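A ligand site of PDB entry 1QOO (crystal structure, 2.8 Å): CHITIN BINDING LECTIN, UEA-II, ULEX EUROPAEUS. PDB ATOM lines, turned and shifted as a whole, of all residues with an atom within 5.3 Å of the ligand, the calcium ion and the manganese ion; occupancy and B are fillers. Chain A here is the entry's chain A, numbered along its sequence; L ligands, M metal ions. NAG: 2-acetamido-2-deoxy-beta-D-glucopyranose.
The side-chain carboxylate (OD1) of Asp 86 sits at hydrogen-bond distance from an oxygen (O6) of the ligand, at 2.7 Å.
O1 of the ligand sits at hydrogen-bond distance from O of Gly 219, 3.0 Å away.
An oxygen (O3) of the ligand sits at hydrogen-bond distance from the backbone NH (N) of Gly 106, 2.9 Å away.
OG of Ser 104 lies within hydrogen-bond range of O3 of the ligand (3.2 Å).
O4 of the ligand is in hydrogen-bond range of ND2 of Asn 136 (3.3 Å).
N of Tyr 130 sits at hydrogen-bond distance from O of Asp 86, 3.4 Å away.
The side-chain carboxylate of Asp 86 is in hydrogen-bond range of the backbone NH of Gly 219, 3.0 Å away.
Val 85 touches the ligand (CG2 to O6, 3.5 Å).
Ala 105 touches the ligand (N to O3, 3.6 Å).
CG of Tyr 135 touches C5 of the ligand (3.98 Å).
N of Asn 220 touches O6 of the ligand, at 3.5 Å.
Hydrophobic or aromatic side chains that line the ligand: Val 85, Tyr 130 and Tyr 135.
Within 4 Å of the ligand: Val 85, Asp 86, Ser 104, Ala 105, Gly 106, Tyr 130, Tyr 135, Asn 136, Gly 219 and Asn 220.
The nearest printed residue that does not touch the ligand is Met 107 (4.9 Å).
Of the 23 residues printed, 4 come within 4 Å of the calcium ion.
OG of Ser 154 touches the manganese ion (3.9 Å).
Five residues have an atom within 4 Å of the manganese ion: Glu 126, Asp 128, Asp 139, His 144 and Ser 154.
The nearest printed residue that does not touch the manganese ion is Ile 152 (4.4 Å).
The calcium ion is bound by the side-chain carboxylate (OD1) of Asp 128 (2.3 Å).
OD1 of Asn 136 is bound to the calcium ion, at 2.5 Å.
O of Tyr 130 is bound to the calcium ion (2.5 Å).
The side-chain carboxylate (OD2) of Asp 139 binds the calcium ion, at 2.6 Å.
The side-chain carboxylate (OD2) of Asp 128 binds the calcium ion.
The calcium ion has five donor atoms within binding distance.
The manganese ion is bound by the side-chain carboxylate of Asp 139 (2.0 Å), the side-chain carboxylate of Glu 126 (2.1 Å), a ring nitrogen (NE2) of His 144 (2.1 Å) and the side-chain carboxylate of Asp 128 (2.2 Å).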
ATOM      1  N   THR A  45      23.433 -18.306   5.261  1.00  0.00           N
ATOM      2  CA  THR A  45      22.672 -19.472   5.718  1.00  0.00           C
ATOM      3  C   THR A  45      23.280 -20.666   4.989  1.00  0.00           C
ATOM      4  O   THR A  45      23.604 -20.561   3.807  1.00  0.00           O
ATOM      5  CB  THR A  45      21.165 -19.365   5.356  1.00  0.00           C
ATOM      6  OG1 THR A  45      20.527 -18.409   6.218  1.00  0.00           O
ATOM      7  CG2 THR A  45      20.472 -20.718   5.485  1.00  0.00           C
ATOM      8  N   VAL A  85      25.136 -20.724  15.760  1.00  0.00           N
ATOM      9  CA  VAL A  85      24.127 -21.702  15.379  1.00  0.00           C
ATOM     10  C   VAL A  85      24.662 -22.476  14.162  1.00  0.00           C
ATOM     11  O   VAL A  85      25.552 -21.988  13.474  1.00  0.00           O
ATOM     12  CB  VAL A  85      22.817 -20.986  15.000  1.00  0.00           C
ATOM     13  CG1 VAL A  85      22.305 -20.196  16.193  1.00  0.00           C
ATOM     14  CG2 VAL A  85      23.031 -20.047  13.820  1.00  0.00           C
ATOM     15  N   ASP A  86      24.165 -23.682  13.885  1.00  0.00           N
ATOM     16  CA  ASP A  86      23.130 -24.379  14.631  1.00  0.00           C
ATOM     17  C   ASP A  86      23.672 -25.644  15.297  1.00  0.00           C
ATOM     18  O   ASP A  86      23.113 -26.116  16.291  1.00  0.00           O
ATOM     19  CB  ASP A  86      22.031 -24.813  13.659  1.00  0.00           C
ATOM     20  CG  ASP A  86      20.815 -23.937  13.758  1.00  0.00           C
ATOM     21  OD1 ASP A  86      20.774 -22.910  13.067  1.00  0.00           O
ATOM     22  OD2 ASP A  86      19.909 -24.298  14.536  1.00  0.00           O
ATOM     23  N   SER A 104      15.864 -27.886   7.310  1.00  0.00           N
ATOM     24  CA  SER A 104      16.376 -26.633   7.826  1.00  0.00           C
ATOM     25  C   SER A 104      17.639 -26.873   8.621  1.00  0.00           C
ATOM     26  O   SER A 104      17.962 -28.011   8.982  1.00  0.00           O
ATOM     27  CB  SER A 104      15.314 -25.937   8.676  1.00  0.00           C
ATOM     28  OG  SER A 104      14.973 -26.707   9.819  1.00  0.00           O
ATOM     29  N   ALA A 105      18.375 -25.801   8.888  1.00  0.00           N
ATOM     30  CA  ALA A 105      19.625 -25.886   9.631  1.00  0.00           C
ATOM     31  C   ALA A 105      19.438 -26.514  11.010  1.00  0.00           C
ATOM     32  O   ALA A 105      20.272 -27.310  11.459  1.00  0.00           O
ATOM     33  CB  ALA A 105      20.237 -24.511   9.755  1.00  0.00           C
ATOM     34  N   GLY A 106      18.327 -26.189  11.656  1.00  0.00           N
ATOM     35  CA  GLY A 106      18.040 -26.723  12.976  1.00  0.00           C
ATOM     36  C   GLY A 106      17.795 -28.207  13.005  1.00  0.00           C
ATOM     37  O   GLY A 106      17.713 -28.817  14.086  1.00  0.00           O
ATOM     38  N   MET A 107      17.621 -28.798  11.824  1.00  0.00           N
ATOM     39  CA  MET A 107      17.411 -30.229  11.694  1.00  0.00           C
ATOM     40  C   MET A 107      18.629 -30.890  11.053  1.00  0.00           C
ATOM     41  O   MET A 107      18.616 -32.072  10.706  1.00  0.00           O
ATOM     42  CB  MET A 107      16.125 -30.513  10.938  1.00  0.00           C
ATOM     43  CG  MET A 107      14.932 -29.983  11.690  1.00  0.00           C
ATOM     44  SD  MET A 107      13.358 -30.345  10.967  1.00  0.00           S
ATOM     45  CE  MET A 107      13.320 -29.190   9.574  1.00  0.00           C
ATOM     46  N   PHE A 108      19.690 -30.089  10.907  1.00  0.00           N
ATOM     47  CA  PHE A 108      20.981 -30.526  10.360  1.00  0.00           C
ATOM     48  C   PHE A 108      20.899 -31.236   9.018  1.00  0.00           C
ATOM     49  O   PHE A 108      21.738 -32.090   8.721  1.00  0.00           O
ATOM     50  CB  PHE A 108      21.681 -31.417  11.388  1.00  0.00           C
ATOM     51  CG  PHE A 108      21.695 -30.851  12.784  1.00  0.00           C
ATOM     52  CD1 PHE A 108      22.353 -29.654  13.068  1.00  0.00           C
ATOM     53  CD2 PHE A 108      21.022 -31.507  13.820  1.00  0.00           C
ATOM     54  CE1 PHE A 108      22.341 -29.120  14.358  1.00  0.00           C
ATOM     55  CE2 PHE A 108      21.011 -30.974  15.120  1.00  0.00           C
ATOM     56  CZ  PHE A 108      21.675 -29.783  15.393  1.00  0.00           C
ATOM     57  N   GLU A 126      24.046 -35.546  17.769  1.00  0.00           N
ATOM     58  CA  GLU A 126      24.114 -34.122  17.515  1.00  0.00           C
ATOM     59  C   GLU A 126      24.883 -33.337  18.554  1.00  0.00           C
ATOM     60  O   GLU A 126      24.906 -33.684  19.733  1.00  0.00           O
ATOM     61  CB  GLU A 126      22.694 -33.538  17.409  1.00  0.00           C
ATOM     62  CG  GLU A 126      21.816 -33.783  18.624  1.00  0.00           C
ATOM     63  CD  GLU A 126      20.605 -32.879  18.681  1.00  0.00           C
ATOM     64  OE1 GLU A 126      19.758 -32.953  17.764  1.00  0.00           O
ATOM     65  OE2 GLU A 126      20.489 -32.084  19.634  1.00  0.00           O
ATOM     66  N   ASP A 128      24.474 -29.881  19.299  1.00  0.00           N
ATOM     67  CA  ASP A 128      23.538 -28.759  19.158  1.00  0.00           C
ATOM     68  C   ASP A 128      23.941 -27.482  19.881  1.00  0.00           C
ATOM     69  O   ASP A 128      23.958 -27.437  21.111  1.00  0.00           O
ATOM     70  CB  ASP A 128      22.194 -29.248  19.700  1.00  0.00           C
ATOM     71  CG  ASP A 128      21.010 -28.591  19.052  1.00  0.00           C
ATOM     72  OD1 ASP A 128      21.144 -27.462  18.514  1.00  0.00           O
ATOM     73  OD2 ASP A 128      19.921 -29.204  19.116  1.00  0.00           O
ATOM     74  N   TYR A 130      22.381 -24.350  19.144  1.00  0.00           N
ATOM     75  CA  TYR A 130      21.210 -23.483  19.257  1.00  0.00           C
ATOM     76  C   TYR A 130      20.043 -24.234  19.892  1.00  0.00           C
ATOM     77  O   TYR A 130      19.638 -25.309  19.426  1.00  0.00           O
ATOM     78  CB  TYR A 130      20.817 -22.942  17.873  1.00  0.00           C
ATOM     79  CG  TYR A 130      19.562 -22.087  17.887  1.00  0.00           C
ATOM     80  CD1 TYR A 130      19.599 -20.759  18.317  1.00  0.00           C
ATOM     81  CD2 TYR A 130      18.330 -22.615  17.493  1.00  0.00           C
ATOM     82  CE1 TYR A 130      18.435 -19.984  18.351  1.00  0.00           C
ATOM     83  CE2 TYR A 130      17.161 -21.849  17.528  1.00  0.00           C
ATOM     84  CZ  TYR A 130      17.221 -20.539  17.955  1.00  0.00           C
ATOM     85  OH  TYR A 130      16.050 -19.794  18.011  1.00  0.00           O
ATOM     86  N   PHE A 131      19.483 -23.643  20.935  1.00  0.00           N
ATOM     87  CA  PHE A 131      18.373 -24.251  21.639  1.00  0.00           C
ATOM     88  C   PHE A 131      17.211 -23.275  21.848  1.00  0.00           C
ATOM     89  O   PHE A 131      16.358 -23.486  22.725  1.00  0.00           O
ATOM     90  CB  PHE A 131      18.869 -24.801  22.978  1.00  0.00           C
ATOM     91  CG  PHE A 131      19.566 -23.771  23.828  1.00  0.00           C
ATOM     92  CD1 PHE A 131      20.931 -23.545  23.706  1.00  0.00           C
ATOM     93  CD2 PHE A 131      18.852 -23.016  24.747  1.00  0.00           C
ATOM     94  CE1 PHE A 131      21.584 -22.592  24.483  1.00  0.00           C
ATOM     95  CE2 PHE A 131      19.491 -22.050  25.537  1.00  0.00           C
ATOM     96  CZ  PHE A 131      20.857 -21.839  25.405  1.00  0.00           C
ATOM     97  N   TYR A 135      12.647 -21.186  17.551  1.00  0.00           N
ATOM     98  CA  TYR A 135      12.772 -22.103  16.408  1.00  0.00           C
ATOM     99  C   TYR A 135      12.962 -23.594  16.698  1.00  0.00           C
ATOM    100  O   TYR A 135      12.669 -24.417  15.834  1.00  0.00           O
ATOM    101  CB  TYR A 135      13.889 -21.661  15.466  1.00  0.00           C
ATOM    102  CG  TYR A 135      13.604 -20.408  14.682  1.00  0.00           C
ATOM    103  CD1 TYR A 135      12.859 -20.444  13.507  1.00  0.00           C
ATOM    104  CD2 TYR A 135      14.120 -19.185  15.097  1.00  0.00           C
ATOM    105  CE1 TYR A 135      12.648 -19.281  12.755  1.00  0.00           C
ATOM    106  CE2 TYR A 135      13.920 -18.028  14.364  1.00  0.00           C
ATOM    107  CZ  TYR A 135      13.192 -18.075  13.197  1.00  0.00           C
ATOM    108  OH  TYR A 135      13.044 -16.933  12.467  1.00  0.00           O
ATOM    109  N   ASN A 136      13.488 -23.950  17.866  1.00  0.00           N
ATOM    110  CA  ASN A 136      13.708 -25.350  18.239  1.00  0.00           C
ATOM    111  C   ASN A 136      13.021 -25.663  19.570  1.00  0.00           C
ATOM    112  O   ASN A 136      13.692 -25.924  20.583  1.00  0.00           O
ATOM    113  CB  ASN A 136      15.205 -25.667  18.407  1.00  0.00           C
ATOM    114  CG  ASN A 136      16.012 -25.424  17.151  1.00  0.00           C
ATOM    115  OD1 ASN A 136      17.237 -25.342  17.225  1.00  0.00           O
ATOM    116  ND2 ASN A 136      15.357 -25.334  16.010  1.00  0.00           N
ATOM    117  N   TRP A 138      11.792 -28.234  20.661  1.00  0.00           N
ATOM    118  CA  TRP A 138      12.114 -29.585  21.130  1.00  0.00           C
ATOM    119  C   TRP A 138      13.407 -29.692  21.948  1.00  0.00           C
ATOM    120  O   TRP A 138      13.637 -30.704  22.611  1.00  0.00           O
ATOM    121  CB  TRP A 138      12.229 -30.504  19.918  1.00  0.00           C
ATOM    122  CG  TRP A 138      13.209 -29.980  18.902  1.00  0.00           C
ATOM    123  CD1 TRP A 138      14.573 -30.059  18.951  1.00  0.00           C
ATOM    124  CD2 TRP A 138      12.887 -29.264  17.704  1.00  0.00           C
ATOM    125  NE1 TRP A 138      15.119 -29.426  17.863  1.00  0.00           N
ATOM    126  CE2 TRP A 138      14.115 -28.926  17.083  1.00  0.00           C
ATOM    127  CE3 TRP A 138      11.691 -28.872  17.097  1.00  0.00           C
ATOM    128  CZ2 TRP A 138      14.173 -28.212  15.881  1.00  0.00           C
ATOM    129  CZ3 TRP A 138      11.755 -28.151  15.894  1.00  0.00           C
ATOM    130  CH2 TRP A 138      12.991 -27.839  15.302  1.00  0.00           C
ATOM    131  N   ASP A 139      14.271 -28.680  21.864  1.00  0.00           N
ATOM    132  CA  ASP A 139      15.553 -28.669  22.559  1.00  0.00           C
ATOM    133  C   ASP A 139      15.484 -28.283  24.023  1.00  0.00           C
ATOM    134  O   ASP A 139      14.548 -27.604  24.441  1.00  0.00           O
ATOM    135  CB  ASP A 139      16.509 -27.674  21.866  1.00  0.00           C
ATOM    136  CG  ASP A 139      17.225 -28.268  20.659  1.00  0.00           C
ATOM    137  OD1 ASP A 139      17.468 -29.500  20.640  1.00  0.00           O
ATOM    138  OD2 ASP A 139      17.576 -27.487  19.736  1.00  0.00           O
ATOM    139  N   PRO A 140      16.436 -28.775  24.840  1.00  0.00           N
ATOM    140  CA  PRO A 140      16.509 -28.464  26.276  1.00  0.00           C
ATOM    141  C   PRO A 140      17.110 -27.055  26.401  1.00  0.00           C
ATOM    142  O   PRO A 140      17.560 -26.490  25.389  1.00  0.00           O
ATOM    143  CB  PRO A 140      17.435 -29.547  26.822  1.00  0.00           C
ATOM    144  CG  PRO A 140      18.310 -29.850  25.664  1.00  0.00           C
ATOM    145  CD  PRO A 140      17.341 -29.899  24.521  1.00  0.00           C
ATOM    146  N   HIS A 144      23.808 -28.814  23.871  1.00  0.00           N
ATOM    147  CA  HIS A 144      23.820 -30.219  24.245  1.00  0.00           C
ATOM    148  C   HIS A 144      24.348 -31.227  23.228  1.00  0.00           C
ATOM    149  O   HIS A 144      24.553 -30.901  22.057  1.00  0.00           O
ATOM    150  CB  HIS A 144      22.379 -30.609  24.595  1.00  0.00           C
ATOM    151  CG  HIS A 144      21.396 -30.245  23.513  1.00  0.00           C
ATOM    152  ND1 HIS A 144      20.963 -28.962  23.305  1.00  0.00           N
ATOM    153  CD2 HIS A 144      20.814 -30.998  22.547  1.00  0.00           C
ATOM    154  CE1 HIS A 144      20.163 -28.924  22.257  1.00  0.00           C
ATOM    155  NE2 HIS A 144      20.048 -30.148  21.773  1.00  0.00           N
ATOM    156  N   ILE A 152      14.373 -35.241  15.422  1.00  0.00           N
ATOM    157  CA  ILE A 152      15.257 -34.171  15.860  1.00  0.00           C
ATOM    158  C   ILE A 152      15.109 -33.922  17.360  1.00  0.00           C
ATOM    159  O   ILE A 152      15.884 -33.177  17.964  1.00  0.00           O
ATOM    160  CB  ILE A 152      14.992 -32.873  15.051  1.00  0.00           C
ATOM    161  CG1 ILE A 152      16.129 -31.867  15.252  1.00  0.00           C
ATOM    162  CG2 ILE A 152      13.665 -32.279  15.437  1.00  0.00           C
ATOM    163  CD1 ILE A 152      17.504 -32.362  14.837  1.00  0.00           C
ATOM    164  N   SER A 154      15.772 -35.393  20.481  1.00  0.00           N
ATOM    165  CA  SER A 154      16.659 -36.402  21.061  1.00  0.00           C
ATOM    166  C   SER A 154      15.985 -37.257  22.123  1.00  0.00           C
ATOM    167  O   SER A 154      15.143 -36.769  22.877  1.00  0.00           O
ATOM    168  CB  SER A 154      17.870 -35.723  21.685  1.00  0.00           C
ATOM    169  OG  SER A 154      18.376 -34.679  20.864  1.00  0.00           O
ATOM    170  N   VAL A 218      23.698 -23.719   9.516  1.00  0.00           N
ATOM    171  CA  VAL A 218      23.773 -22.356  10.041  1.00  0.00           C
ATOM    172  C   VAL A 218      22.468 -21.734   9.574  1.00  0.00           C
ATOM    173  O   VAL A 218      22.301 -21.440   8.397  1.00  0.00           O
ATOM    174  CB  VAL A 218      24.983 -21.578   9.470  1.00  0.00           C
ATOM    175  CG1 VAL A 218      24.972 -20.141   9.965  1.00  0.00           C
ATOM    176  CG2 VAL A 218      26.286 -22.244   9.889  1.00  0.00           C
ATOM    177  N   GLY A 219      21.522 -21.599  10.495  1.00  0.00           N
ATOM    178  CA  GLY A 219      20.223 -21.052  10.150  1.00  0.00           C
ATOM    179  C   GLY A 219      20.119 -19.555  10.111  1.00  0.00           C
ATOM    180  O   GLY A 219      19.247 -19.016   9.432  1.00  0.00           O
ATOM    181  N   ASN A 220      21.014 -18.886  10.832  1.00  0.00           N
ATOM    182  CA  ASN A 220      21.018 -17.431  10.899  1.00  0.00           C
ATOM    183  C   ASN A 220      22.430 -16.887  10.680  1.00  0.00           C
ATOM    184  O   ASN A 220      23.278 -16.970  11.571  1.00  0.00           O
ATOM    185  CB  ASN A 220      20.449 -16.981  12.252  1.00  0.00           C
ATOM    186  CG  ASN A 220      20.441 -15.476  12.431  1.00  0.00           C
ATOM    187  OD1 ASN A 220      20.481 -14.981  13.553  1.00  0.00           O
ATOM    188  ND2 ASN A 220      20.395 -14.732  11.324  1.00  0.00           N
HETATM  189  C1  NAG L   1      16.242 -20.389  11.300  1.00  0.00           C
HETATM  190  C2  NAG L   1      16.185 -21.799  10.713  1.00  0.00           C
HETATM  191  C3  NAG L   1      16.162 -22.844  11.828  1.00  0.00           C
HETATM  192  C4  NAG L   1      17.318 -22.596  12.797  1.00  0.00           C
HETATM  193  C5  NAG L   1      17.258 -21.158  13.299  1.00  0.00           C
HETATM  194  C6  NAG L   1      18.353 -20.811  14.273  1.00  0.00           C
HETATM  195  C7  NAG L   1      15.093 -21.704   8.563  1.00  0.00           C
HETATM  196  C8  NAG L   1      13.811 -21.845   7.761  1.00  0.00           C
HETATM  197  N2  NAG L   1      15.002 -21.907   9.875  1.00  0.00           N
HETATM  198  O1  NAG L   1      16.410 -19.467  10.278  1.00  0.00           O
HETATM  199  O3  NAG L   1      16.271 -24.162  11.275  1.00  0.00           O
HETATM  200  O4  NAG L   1      17.206 -23.481  13.931  1.00  0.00           O
HETATM  201  O5  NAG L   1      17.358 -20.261  12.187  1.00  0.00           O
HETATM  202  O6  NAG L   1      19.575 -20.566  13.585  1.00  0.00           O
HETATM  203  O7  NAG L   1      16.156 -21.421   7.997  1.00  0.00           O
HETATM  204 CA    CA M   1      19.016 -26.982  17.665  1.00  0.00          CA
HETATM  205 MN    MN M   2      18.902 -30.845  20.109  1.00  0.00          MN
